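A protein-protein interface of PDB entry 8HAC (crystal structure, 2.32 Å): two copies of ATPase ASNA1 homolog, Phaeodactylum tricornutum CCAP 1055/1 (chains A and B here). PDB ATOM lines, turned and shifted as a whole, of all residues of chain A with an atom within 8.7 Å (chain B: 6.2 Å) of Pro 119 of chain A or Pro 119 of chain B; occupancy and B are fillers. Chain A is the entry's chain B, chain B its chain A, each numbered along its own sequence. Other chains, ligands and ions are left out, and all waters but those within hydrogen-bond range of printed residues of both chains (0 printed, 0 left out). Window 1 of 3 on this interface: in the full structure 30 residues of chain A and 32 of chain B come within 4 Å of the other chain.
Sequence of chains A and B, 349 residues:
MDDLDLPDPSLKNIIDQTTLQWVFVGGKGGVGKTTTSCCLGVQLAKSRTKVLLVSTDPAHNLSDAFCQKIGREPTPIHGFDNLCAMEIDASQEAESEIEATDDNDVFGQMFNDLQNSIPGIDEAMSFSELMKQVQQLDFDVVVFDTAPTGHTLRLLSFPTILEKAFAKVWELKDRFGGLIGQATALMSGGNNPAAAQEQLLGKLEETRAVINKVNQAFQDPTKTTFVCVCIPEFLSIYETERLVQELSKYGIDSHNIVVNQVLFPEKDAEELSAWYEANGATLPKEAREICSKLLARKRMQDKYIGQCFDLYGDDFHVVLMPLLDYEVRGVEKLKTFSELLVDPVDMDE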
ATOM      1  N   ASP A 113     -24.545 -16.944  17.245  1.00  0.00           N
ATOM      2  CA  ASP A 113     -23.272 -17.048  16.539  1.00  0.00           C
ATOM      3  C   ASP A 113     -22.687 -18.440  16.669  1.00  0.00           C
ATOM      4  O   ASP A 113     -22.150 -18.991  15.703  1.00  0.00           O
ATOM      5  CB  ASP A 113     -22.283 -16.020  17.086  1.00  0.00           C
ATOM      6  CG  ASP A 113     -22.710 -14.600  16.812  1.00  0.00           C
ATOM      7  OD1 ASP A 113     -23.657 -14.408  16.018  1.00  0.00           O
ATOM      8  OD2 ASP A 113     -22.107 -13.679  17.407  1.00  0.00           O
ATOM      9  N   LEU A 114     -22.774 -19.022  17.865  1.00  0.00           N
ATOM     10  CA  LEU A 114     -22.252 -20.368  18.056  1.00  0.00           C
ATOM     11  C   LEU A 114     -23.055 -21.381  17.251  1.00  0.00           C
ATOM     12  O   LEU A 114     -22.482 -22.282  16.630  1.00  0.00           O
ATOM     13  CB  LEU A 114     -22.254 -20.730  19.538  1.00  0.00           C
ATOM     14  CG  LEU A 114     -21.598 -22.073  19.857  1.00  0.00           C
ATOM     15  CD1 LEU A 114     -20.121 -22.057  19.476  1.00  0.00           C
ATOM     16  CD2 LEU A 114     -21.792 -22.433  21.324  1.00  0.00           C
ATOM     17  N   GLN A 115     -24.380 -21.239  17.235  1.00  0.00           N
ATOM     18  CA  GLN A 115     -25.200 -22.153  16.444  1.00  0.00           C
ATOM     19  C   GLN A 115     -24.833 -22.084  14.967  1.00  0.00           C
ATOM     20  O   GLN A 115     -24.751 -23.118  14.295  1.00  0.00           O
ATOM     21  CB  GLN A 115     -26.682 -21.843  16.644  1.00  0.00           C
ATOM     22  CG  GLN A 115     -27.206 -22.237  18.014  1.00  0.00           C
ATOM     23  CD  GLN A 115     -28.683 -21.940  18.175  1.00  0.00           C
ATOM     24  OE1 GLN A 115     -29.441 -22.774  18.670  1.00  0.00           O
ATOM     25  NE2 GLN A 115     -29.100 -20.746  17.759  1.00  0.00           N
ATOM     26  N   ASN A 116     -24.581 -20.874  14.454  1.00  0.00           N
ATOM     27  CA  ASN A 116     -24.182 -20.727  13.055  1.00  0.00           C
ATOM     28  C   ASN A 116     -22.776 -21.259  12.801  1.00  0.00           C
ATOM     29  O   ASN A 116     -22.511 -21.820  11.730  1.00  0.00           O
ATOM     30  CB  ASN A 116     -24.271 -19.259  12.639  1.00  0.00           C
ATOM     31  CG  ASN A 116     -25.696 -18.812  12.378  1.00  0.00           C
ATOM     32  OD1 ASN A 116     -26.463 -19.511  11.716  1.00  0.00           O
ATOM     33  ND2 ASN A 116     -26.065 -17.653  12.918  1.00  0.00           N
ATOM     34  N   SER A 117     -21.876 -21.117  13.776  1.00  0.00           N
ATOM     35  CA  SER A 117     -20.484 -21.531  13.616  1.00  0.00           C
ATOM     36  C   SER A 117     -20.324 -23.043  13.710  1.00  0.00           C
ATOM     37  O   SER A 117     -19.566 -23.641  12.939  1.00  0.00           O
ATOM     38  CB  SER A 117     -19.620 -20.862  14.686  1.00  0.00           C
ATOM     39  OG  SER A 117     -19.256 -19.553  14.308  1.00  0.00           O
ATOM     40  N   ILE A 118     -21.020 -23.673  14.650  1.00  0.00           N
ATOM     41  CA  ILE A 118     -20.852 -25.095  14.936  1.00  0.00           C
ATOM     42  C   ILE A 118     -22.150 -25.821  14.621  1.00  0.00           C
ATOM     43  O   ILE A 118     -22.997 -25.988  15.510  1.00  0.00           O
ATOM     44  CB  ILE A 118     -20.441 -25.335  16.399  1.00  0.00           C
ATOM     45  CG1 ILE A 118     -19.231 -24.477  16.755  1.00  0.00           C
ATOM     46  CG2 ILE A 118     -20.121 -26.811  16.634  1.00  0.00           C
ATOM     47  CD1 ILE A 118     -18.014 -24.826  15.945  1.00  0.00           C
ATOM     48  N   PRO A 119     -22.363 -26.240  13.376  1.00  0.00           N
ATOM     49  CA  PRO A 119     -23.576 -26.997  13.059  1.00  0.00           C
ATOM     50  C   PRO A 119     -23.618 -28.287  13.863  1.00  0.00           C
ATOM     51  O   PRO A 119     -22.631 -29.025  13.944  1.00  0.00           O
ATOM     52  CB  PRO A 119     -23.446 -27.264  11.555  1.00  0.00           C
ATOM     53  CG  PRO A 119     -21.980 -27.167  11.282  1.00  0.00           C
ATOM     54  CD  PRO A 119     -21.476 -26.106  12.208  1.00  0.00           C
ATOM     55  N   GLY A 120     -24.757 -28.529  14.498  1.00  0.00           N
ATOM     56  CA  GLY A 120     -24.944 -29.709  15.313  1.00  0.00           C
ATOM     57  C   GLY A 120     -24.973 -29.448  16.801  1.00  0.00           C
ATOM     58  O   GLY A 120     -25.312 -30.365  17.560  1.00  0.00           O
ATOM     59  N   ILE A 121     -24.616 -28.242  17.255  1.00  0.00           N
ATOM     60  CA  ILE A 121     -24.664 -27.979  18.690  1.00  0.00           C
ATOM     61  C   ILE A 121     -26.115 -27.954  19.167  1.00  0.00           C
ATOM     62  O   ILE A 121     -26.423 -28.425  20.270  1.00  0.00           O
ATOM     63  CB  ILE A 121     -23.910 -26.677  19.038  1.00  0.00           C
ATOM     64  CG1 ILE A 121     -23.817 -26.497  20.556  1.00  0.00           C
ATOM     65  CG2 ILE A 121     -24.570 -25.461  18.401  1.00  0.00           C
ATOM     66  CD1 ILE A 121     -23.026 -27.582  21.237  1.00  0.00           C
ATOM     67  N   ASP A 122     -27.034 -27.462  18.330  1.00  0.00           N
ATOM     68  CA  ASP A 122     -28.444 -27.461  18.705  1.00  0.00           C
ATOM     69  C   ASP A 122     -28.981 -28.883  18.838  1.00  0.00           C
ATOM     70  O   ASP A 122     -29.765 -29.178  19.750  1.00  0.00           O
ATOM     71  CB  ASP A 122     -29.257 -26.671  17.678  1.00  0.00           C
ATOM     72  CG  ASP A 122     -29.082 -27.196  16.254  1.00  0.00           C
ATOM     73  OD1 ASP A 122     -28.224 -28.081  16.019  1.00  0.00           O
ATOM     74  OD2 ASP A 122     -29.815 -26.720  15.362  1.00  0.00           O
ATOM     75  N   GLU A 123     -28.564 -29.779  17.944  1.00  0.00           N
ATOM     76  CA  GLU A 123     -28.957 -31.179  18.061  1.00  0.00           C
ATOM     77  C   GLU A 123     -28.429 -31.784  19.355  1.00  0.00           C
ATOM     78  O   GLU A 123     -29.136 -32.541  20.028  1.00  0.00           O
ATOM     79  CB  GLU A 123     -28.453 -31.959  16.846  1.00  0.00           C
ATOM     80  CG  GLU A 123     -29.384 -31.888  15.645  1.00  0.00           C
ATOM     81  CD  GLU A 123     -28.840 -32.625  14.434  1.00  0.00           C
ATOM     82  OE1 GLU A 123     -27.605 -32.598  14.222  1.00  0.00           O
ATOM     83  OE2 GLU A 123     -29.645 -33.228  13.694  1.00  0.00           O
ATOM     84  N   ALA A 124     -27.185 -31.451  19.721  1.00  0.00           N
ATOM     85  CA  ALA A 124     -26.609 -31.939  20.972  1.00  0.00           C
ATOM     86  C   ALA A 124     -27.392 -31.441  22.185  1.00  0.00           C
ATOM     87  O   ALA A 124     -27.631 -32.199  23.131  1.00  0.00           O
ATOM     88  CB  ALA A 124     -25.139 -31.515  21.075  1.00  0.00           C
ATOM     89  N   ARG A 154     -24.351 -38.589  13.321  1.00  0.00           N
ATOM     90  CA  ARG A 154     -24.025 -37.307  13.952  1.00  0.00           C
ATOM     91  C   ARG A 154     -24.344 -37.324  15.441  1.00  0.00           C
ATOM     92  O   ARG A 154     -23.590 -36.758  16.260  1.00  0.00           O
ATOM     93  CB  ARG A 154     -24.775 -36.162  13.272  1.00  0.00           C
ATOM     94  CG  ARG A 154     -24.095 -35.590  12.049  1.00  0.00           C
ATOM     95  CD  ARG A 154     -24.538 -34.147  11.831  1.00  0.00           C
ATOM     96  NE  ARG A 154     -25.969 -33.979  12.065  1.00  0.00           N
ATOM     97  CZ  ARG A 154     -26.910 -34.231  11.162  1.00  0.00           C
ATOM     98  NH1 ARG A 154     -26.603 -34.652   9.945  1.00  0.00           N
ATOM     99  NH2 ARG A 154     -28.189 -34.063  11.490  1.00  0.00           N
ATOM    100  N   SER A 157     -21.505 -38.463  16.986  1.00  0.00           N
ATOM    101  CA  SER A 157     -20.391 -37.511  16.982  1.00  0.00           C
ATOM    102  C   SER A 157     -20.558 -36.353  17.969  1.00  0.00           C
ATOM    103  O   SER A 157     -19.661 -35.506  18.048  1.00  0.00           O
ATOM    104  CB  SER A 157     -20.182 -36.932  15.581  1.00  0.00           C
ATOM    105  OG  SER A 157     -21.143 -35.929  15.308  1.00  0.00           O
ATOM    106  N   PHE A 158     -21.691 -36.254  18.666  1.00  0.00           N
ATOM    107  CA  PHE A 158     -21.935 -35.156  19.622  1.00  0.00           C
ATOM    108  C   PHE A 158     -20.742 -34.722  20.489  1.00  0.00           C
ATOM    109  O   PHE A 158     -20.561 -33.515  20.695  1.00  0.00           O
ATOM    110  CB  PHE A 158     -23.089 -35.510  20.571  1.00  0.00           C
ATOM    111  CG  PHE A 158     -24.448 -35.329  19.967  1.00  0.00           C
ATOM    112  CD1 PHE A 158     -24.610 -34.593  18.801  1.00  0.00           C
ATOM    113  CD2 PHE A 158     -25.560 -35.908  20.551  1.00  0.00           C
ATOM    114  CE1 PHE A 158     -25.858 -34.432  18.233  1.00  0.00           C
ATOM    115  CE2 PHE A 158     -26.810 -35.752  19.986  1.00  0.00           C
ATOM    116  CZ  PHE A 158     -26.960 -35.012  18.827  1.00  0.00           C
ATOM    117  N   THR A 160     -17.535 -34.677  19.864  1.00  0.00           N
ATOM    118  CA  THR A 160     -16.688 -33.857  19.004  1.00  0.00           C
ATOM    119  C   THR A 160     -17.322 -32.497  18.729  1.00  0.00           C
ATOM    120  O   THR A 160     -16.630 -31.468  18.720  1.00  0.00           O
ATOM    121  CB  THR A 160     -16.416 -34.600  17.695  1.00  0.00           C
ATOM    122  OG1 THR A 160     -15.789 -35.855  17.984  1.00  0.00           O
ATOM    123  CG2 THR A 160     -15.518 -33.785  16.776  1.00  0.00           C
ATOM    124  N   ILE A 161     -18.639 -32.473  18.500  1.00  0.00           N
ATOM    125  CA  ILE A 161     -19.334 -31.211  18.257  1.00  0.00           C
ATOM    126  C   ILE A 161     -19.196 -30.292  19.462  1.00  0.00           C
ATOM    127  O   ILE A 161     -18.927 -29.089  19.323  1.00  0.00           O
ATOM    128  CB  ILE A 161     -20.814 -31.475  17.911  1.00  0.00           C
ATOM    129  CG1 ILE A 161     -20.941 -32.058  16.498  1.00  0.00           C
ATOM    130  CG2 ILE A 161     -21.637 -30.200  18.034  1.00  0.00           C
ATOM    131  CD1 ILE A 161     -22.140 -32.969  16.321  1.00  0.00           C
ATOM    132  N   LEU A 162     -19.349 -30.849  20.665  1.00  0.00           N
ATOM    133  CA  LEU A 162     -19.218 -30.048  21.878  1.00  0.00           C
ATOM    134  C   LEU A 162     -17.790 -29.540  22.058  1.00  0.00           C
ATOM    135  O   LEU A 162     -17.581 -28.393  22.470  1.00  0.00           O
ATOM    136  CB  LEU A 162     -19.662 -30.867  23.090  1.00  0.00           C
ATOM    137  CG  LEU A 162     -21.165 -30.830  23.353  1.00  0.00           C
ATOM    138  CD1 LEU A 162     -21.578 -32.026  24.175  1.00  0.00           C
ATOM    139  CD2 LEU A 162     -21.537 -29.541  24.053  1.00  0.00           C
ATOM    140  N   LYS A 164     -15.620 -28.870  19.713  1.00  0.00           N
ATOM    141  CA  LYS A 164     -15.439 -27.767  18.770  1.00  0.00           C
ATOM    142  C   LYS A 164     -16.185 -26.509  19.212  1.00  0.00           C
ATOM    143  O   LYS A 164     -15.704 -25.396  18.981  1.00  0.00           O
ATOM    144  CB  LYS A 164     -15.882 -28.183  17.365  1.00  0.00           C
ATOM    145  CG  LYS A 164     -14.890 -29.089  16.663  1.00  0.00           C
ATOM    146  CD  LYS A 164     -15.358 -29.547  15.293  1.00  0.00           C
ATOM    147  CE  LYS A 164     -16.862 -29.744  15.227  1.00  0.00           C
ATOM    148  NZ  LYS A 164     -17.530 -28.839  14.252  1.00  0.00           N
ATOM    149  N   ALA A 165     -17.353 -26.658  19.844  1.00  0.00           N
ATOM    150  CA  ALA A 165     -18.073 -25.486  20.342  1.00  0.00           C
ATOM    151  C   ALA A 165     -17.301 -24.802  21.470  1.00  0.00           C
ATOM    152  O   ALA A 165     -17.220 -23.565  21.519  1.00  0.00           O
ATOM    153  CB  ALA A 165     -19.474 -25.885  20.807  1.00  0.00           C
ATOM    154  N   LYS A 168     -14.469 -22.955  19.880  1.00  0.00           N
ATOM    155  CA  LYS A 168     -14.938 -21.721  19.265  1.00  0.00           C
ATOM    156  C   LYS A 168     -15.149 -20.633  20.309  1.00  0.00           C
ATOM    157  O   LYS A 168     -14.750 -19.483  20.103  1.00  0.00           O
ATOM    158  CB  LYS A 168     -16.229 -21.975  18.489  1.00  0.00           C
ATOM    159  CG  LYS A 168     -16.677 -20.802  17.647  1.00  0.00           C
ATOM    160  CD  LYS A 168     -15.678 -20.481  16.539  1.00  0.00           C
ATOM    161  CE  LYS A 168     -15.674 -21.550  15.452  1.00  0.00           C
ATOM    162  NZ  LYS A 168     -14.912 -21.102  14.246  1.00  0.00           N
ATOM    163  N   LEU B 114     -23.434 -37.693   2.576  1.00  0.00           N
ATOM    164  CA  LEU B 114     -22.439 -36.633   2.644  1.00  0.00           C
ATOM    165  C   LEU B 114     -23.025 -35.373   3.272  1.00  0.00           C
ATOM    166  O   LEU B 114     -22.376 -34.733   4.104  1.00  0.00           O
ATOM    167  CB  LEU B 114     -21.888 -36.352   1.249  1.00  0.00           C
ATOM    168  CG  LEU B 114     -20.750 -35.340   1.168  1.00  0.00           C
ATOM    169  CD1 LEU B 114     -19.543 -35.820   1.953  1.00  0.00           C
ATOM    170  CD2 LEU B 114     -20.391 -35.135  -0.288  1.00  0.00           C
ATOM    171  N   GLN B 115     -24.261 -35.020   2.902  1.00  0.00           N
ATOM    172  CA  GLN B 115     -24.926 -33.863   3.497  1.00  0.00           C
ATOM    173  C   GLN B 115     -25.089 -34.029   5.002  1.00  0.00           C
ATOM    174  O   GLN B 115     -24.952 -33.062   5.760  1.00  0.00           O
ATOM    175  CB  GLN B 115     -26.292 -33.642   2.850  1.00  0.00           C
ATOM    176  CG  GLN B 115     -26.262 -33.117   1.434  1.00  0.00           C
ATOM    177  CD  GLN B 115     -27.658 -32.903   0.877  1.00  0.00           C
ATOM    178  OE1 GLN B 115     -28.542 -33.744   1.041  1.00  0.00           O
ATOM    179  NE2 GLN B 115     -27.864 -31.768   0.222  1.00  0.00           N
ATOM    180  N   ASN B 116     -25.415 -35.241   5.452  1.00  0.00           N
ATOM    181  CA  ASN B 116     -25.533 -35.475   6.885  1.00  0.00           C
ATOM    182  C   ASN B 116     -24.173 -35.449   7.575  1.00  0.00           C
ATOM    183  O   ASN B 116     -24.070 -34.990   8.716  1.00  0.00           O
ATOM    184  CB  ASN B 116     -26.240 -36.803   7.144  1.00  0.00           C
ATOM    185  CG  ASN B 116     -27.736 -36.703   6.965  1.00  0.00           C
ATOM    186  OD1 ASN B 116     -28.362 -35.754   7.433  1.00  0.00           O
ATOM    187  ND2 ASN B 116     -28.319 -37.676   6.281  1.00  0.00           N
ATOM    188  N   SER B 117     -23.126 -35.920   6.893  1.00  0.00           N
ATOM    189  CA  SER B 117     -21.791 -35.985   7.478  1.00  0.00           C
ATOM    190  C   SER B 117     -21.108 -34.623   7.503  1.00  0.00           C
ATOM    191  O   SER B 117     -20.454 -34.275   8.493  1.00  0.00           O
ATOM    192  CB  SER B 117     -20.931 -36.978   6.696  1.00  0.00           C
ATOM    193  OG  SER B 117     -21.159 -38.307   7.132  1.00  0.00           O
ATOM    194  N   ILE B 118     -21.225 -33.859   6.420  1.00  0.00           N
ATOM    195  CA  ILE B 118     -20.535 -32.579   6.272  1.00  0.00           C
ATOM    196  C   ILE B 118     -21.586 -31.482   6.134  1.00  0.00           C
ATOM    197  O   ILE B 118     -21.905 -31.072   5.007  1.00  0.00           O
ATOM    198  CB  ILE B 118     -19.596 -32.589   5.056  1.00  0.00           C
ATOM    199  CG1 ILE B 118     -18.715 -33.840   5.061  1.00  0.00           C
ATOM    200  CG2 ILE B 118     -18.720 -31.355   5.052  1.00  0.00           C
ATOM    201  CD1 ILE B 118     -17.779 -33.941   6.238  1.00  0.00           C
ATOM    202  N   PRO B 119     -22.131 -30.966   7.235  1.00  0.00           N
ATOM    203  CA  PRO B 119     -23.128 -29.891   7.131  1.00  0.00           C
ATOM    204  C   PRO B 119     -22.533 -28.666   6.455  1.00  0.00           C
ATOM    205  O   PRO B 119     -21.422 -28.236   6.777  1.00  0.00           O
ATOM    206  CB  PRO B 119     -23.502 -29.613   8.593  1.00  0.00           C
ATOM    207  CG  PRO B 119     -23.130 -30.868   9.327  1.00  0.00           C
ATOM    208  CD  PRO B 119     -21.898 -31.366   8.632  1.00  0.00           C
ATOM    209  N   GLY B 120     -23.261 -28.135   5.474  1.00  0.00           N
ATOM    210  CA  GLY B 120     -22.814 -26.993   4.709  1.00  0.00           C
ATOM    211  C   GLY B 120     -22.397 -27.314   3.292  1.00  0.00           C
ATOM    212  O   GLY B 120     -22.156 -26.379   2.514  1.00  0.00           O
ATOM    213  N   ILE B 121     -22.298 -28.595   2.924  1.00  0.00           N
ATOM    214  CA  ILE B 121     -21.862 -28.941   1.573  1.00  0.00           C
ATOM    215  C   ILE B 121     -22.907 -28.513   0.547  1.00  0.00           C
ATOM    216  O   ILE B 121     -22.567 -28.074  -0.562  1.00  0.00           O
ATOM    217  CB  ILE B 121     -21.537 -30.447   1.477  1.00  0.00           C
ATOM    218  CG1 ILE B 121     -20.967 -30.800   0.095  1.00  0.00           C
ATOM    219  CG2 ILE B 121     -22.764 -31.297   1.764  1.00  0.00           C
ATOM    220  CD1 ILE B 121     -19.652 -30.113  -0.239  1.00  0.00           C
ATOM    221  N   ASP B 122     -24.190 -28.609   0.902  1.00  0.00           N
ATOM    222  CA  ASP B 122     -25.232 -28.178  -0.022  1.00  0.00           C
ATOM    223  C   ASP B 122     -25.206 -26.667  -0.218  1.00  0.00           C
ATOM    224  O   ASP B 122     -25.410 -26.180  -1.338  1.00  0.00           O
ATOM    225  CB  ASP B 122     -26.601 -28.654   0.463  1.00  0.00           C
ATOM    226  CG  ASP B 122     -27.660 -28.565  -0.620  1.00  0.00           C
ATOM    227  OD1 ASP B 122     -27.539 -29.284  -1.643  1.00  0.00           O
ATOM    228  OD2 ASP B 122     -28.607 -27.768  -0.451  1.00  0.00           O
ATOM    229  N   ARG B 154     -19.786 -18.482   7.214  1.00  0.00           N
ATOM    230  CA  ARG B 154     -19.759 -19.840   6.674  1.00  0.00           C
ATOM    231  C   ARG B 154     -19.444 -19.825   5.185  1.00  0.00           C
ATOM    232  O   ARG B 154     -18.703 -20.685   4.684  1.00  0.00           O
ATOM    233  CB  ARG B 154     -21.099 -20.530   6.928  1.00  0.00           C
ATOM    234  CG  ARG B 154     -21.241 -21.138   8.315  1.00  0.00           C
ATOM    235  CD  ARG B 154     -22.252 -22.278   8.308  1.00  0.00           C
ATOM    236  NE  ARG B 154     -23.412 -21.967   7.482  1.00  0.00           N
ATOM    237  CZ  ARG B 154     -24.456 -21.261   7.894  1.00  0.00           C
ATOM    238  NH1 ARG B 154     -24.526 -20.788   9.126  1.00  0.00           N
ATOM    239  NH2 ARG B 154     -25.450 -21.018   7.043  1.00  0.00           N
ATOM    240  N   ILE B 161     -15.005 -26.651   3.721  1.00  0.00           N
ATOM    241  CA  ILE B 161     -16.094 -27.625   3.709  1.00  0.00           C
ATOM    242  C   ILE B 161     -15.963 -28.558   2.510  1.00  0.00           C
ATOM    243  O   ILE B 161     -16.154 -29.776   2.628  1.00  0.00           O
ATOM    244  CB  ILE B 161     -17.451 -26.891   3.726  1.00  0.00           C
ATOM    245  CG1 ILE B 161     -17.726 -26.314   5.121  1.00  0.00           C
ATOM    246  CG2 ILE B 161     -18.585 -27.795   3.251  1.00  0.00           C
ATOM    247  CD1 ILE B 161     -18.569 -25.057   5.100  1.00  0.00           C
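The side-chain carboxylate (OE2) of Glu 123 of chain A lies within salt-bridge range of the guanidinium group (NH2) of Arg 154 of chain A (2.8 Å). The backbone carbonyl oxygen of Arg 154 of chain A sits at hydrogen-bond distance from the side-chain hydroxyl of Ser 157 of chain A.
Asn 116 of chain A touches Arg 154 of chain B, and with the chains exchanged Arg 154 of chain A touches Asn 116 of chain B. Pro 119 of chain B touches its own counterpart, Pro 119 of chain A. Positions printed for both chains: 114, 115, 116, 117, 118, 119, 120, 121, 122, 154 and 161. Of the 3 pairs that touch across the chains among the printed residues, 3 have their exchanged pair printed and touching as well.
CB of Pro 119 of chain A touches CB of Pro 119 of chain B (3.8 Å).
The guanidinium group (NH1) of Arg 154 of chain A is in hydrogen-bond range of the backbone carbonyl oxygen (O) of Asn 116 of chain B (2.8 Å). O of Asn 116 of chain A sits at hydrogen-bond distance from NH1 of Arg 154 of chain B (3.5 Å).
Of the 11 printed residues of chain B, 3 touch a printed residue of chain A. Printed residues of chain B that touch a printed residue of chain A: Asn 116, Pro 119 and Arg 154. Of the 21 printed residues of chain A, 3 touch a printed residue of chain B. Hydrophobic or aromatic side chains of chain A within 4 Å of the printed part of chain B: Pro 119. Among the printed residues, no Asp or Glu carboxylate lies within 4 Å of a Lys or Arg side-chain nitrogen of the other chain.
Of the printed residues of chain B, Asn 116 of chain A touches Arg 154. Pro 119 of chain A touches one residue of chain B. Printed residues of chain B within 4 Å of Arg 154 of chain A: Asn 116. Pro 119 of chain B touches one residue of chain A. No residue of chain A comes within 4 Å of Gly 120 of chain B. Printed residues of chain A within 4 Å of Arg 154 of chain B: Asn 116. The nearest residue of chain B that does not touch Pro 119 of chain A is Arg 154 of chain B (5.5 Å). The nearest residue of chain A that does not touch Pro 119 of chain B is Arg 154 of chain A (4.4 Å).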
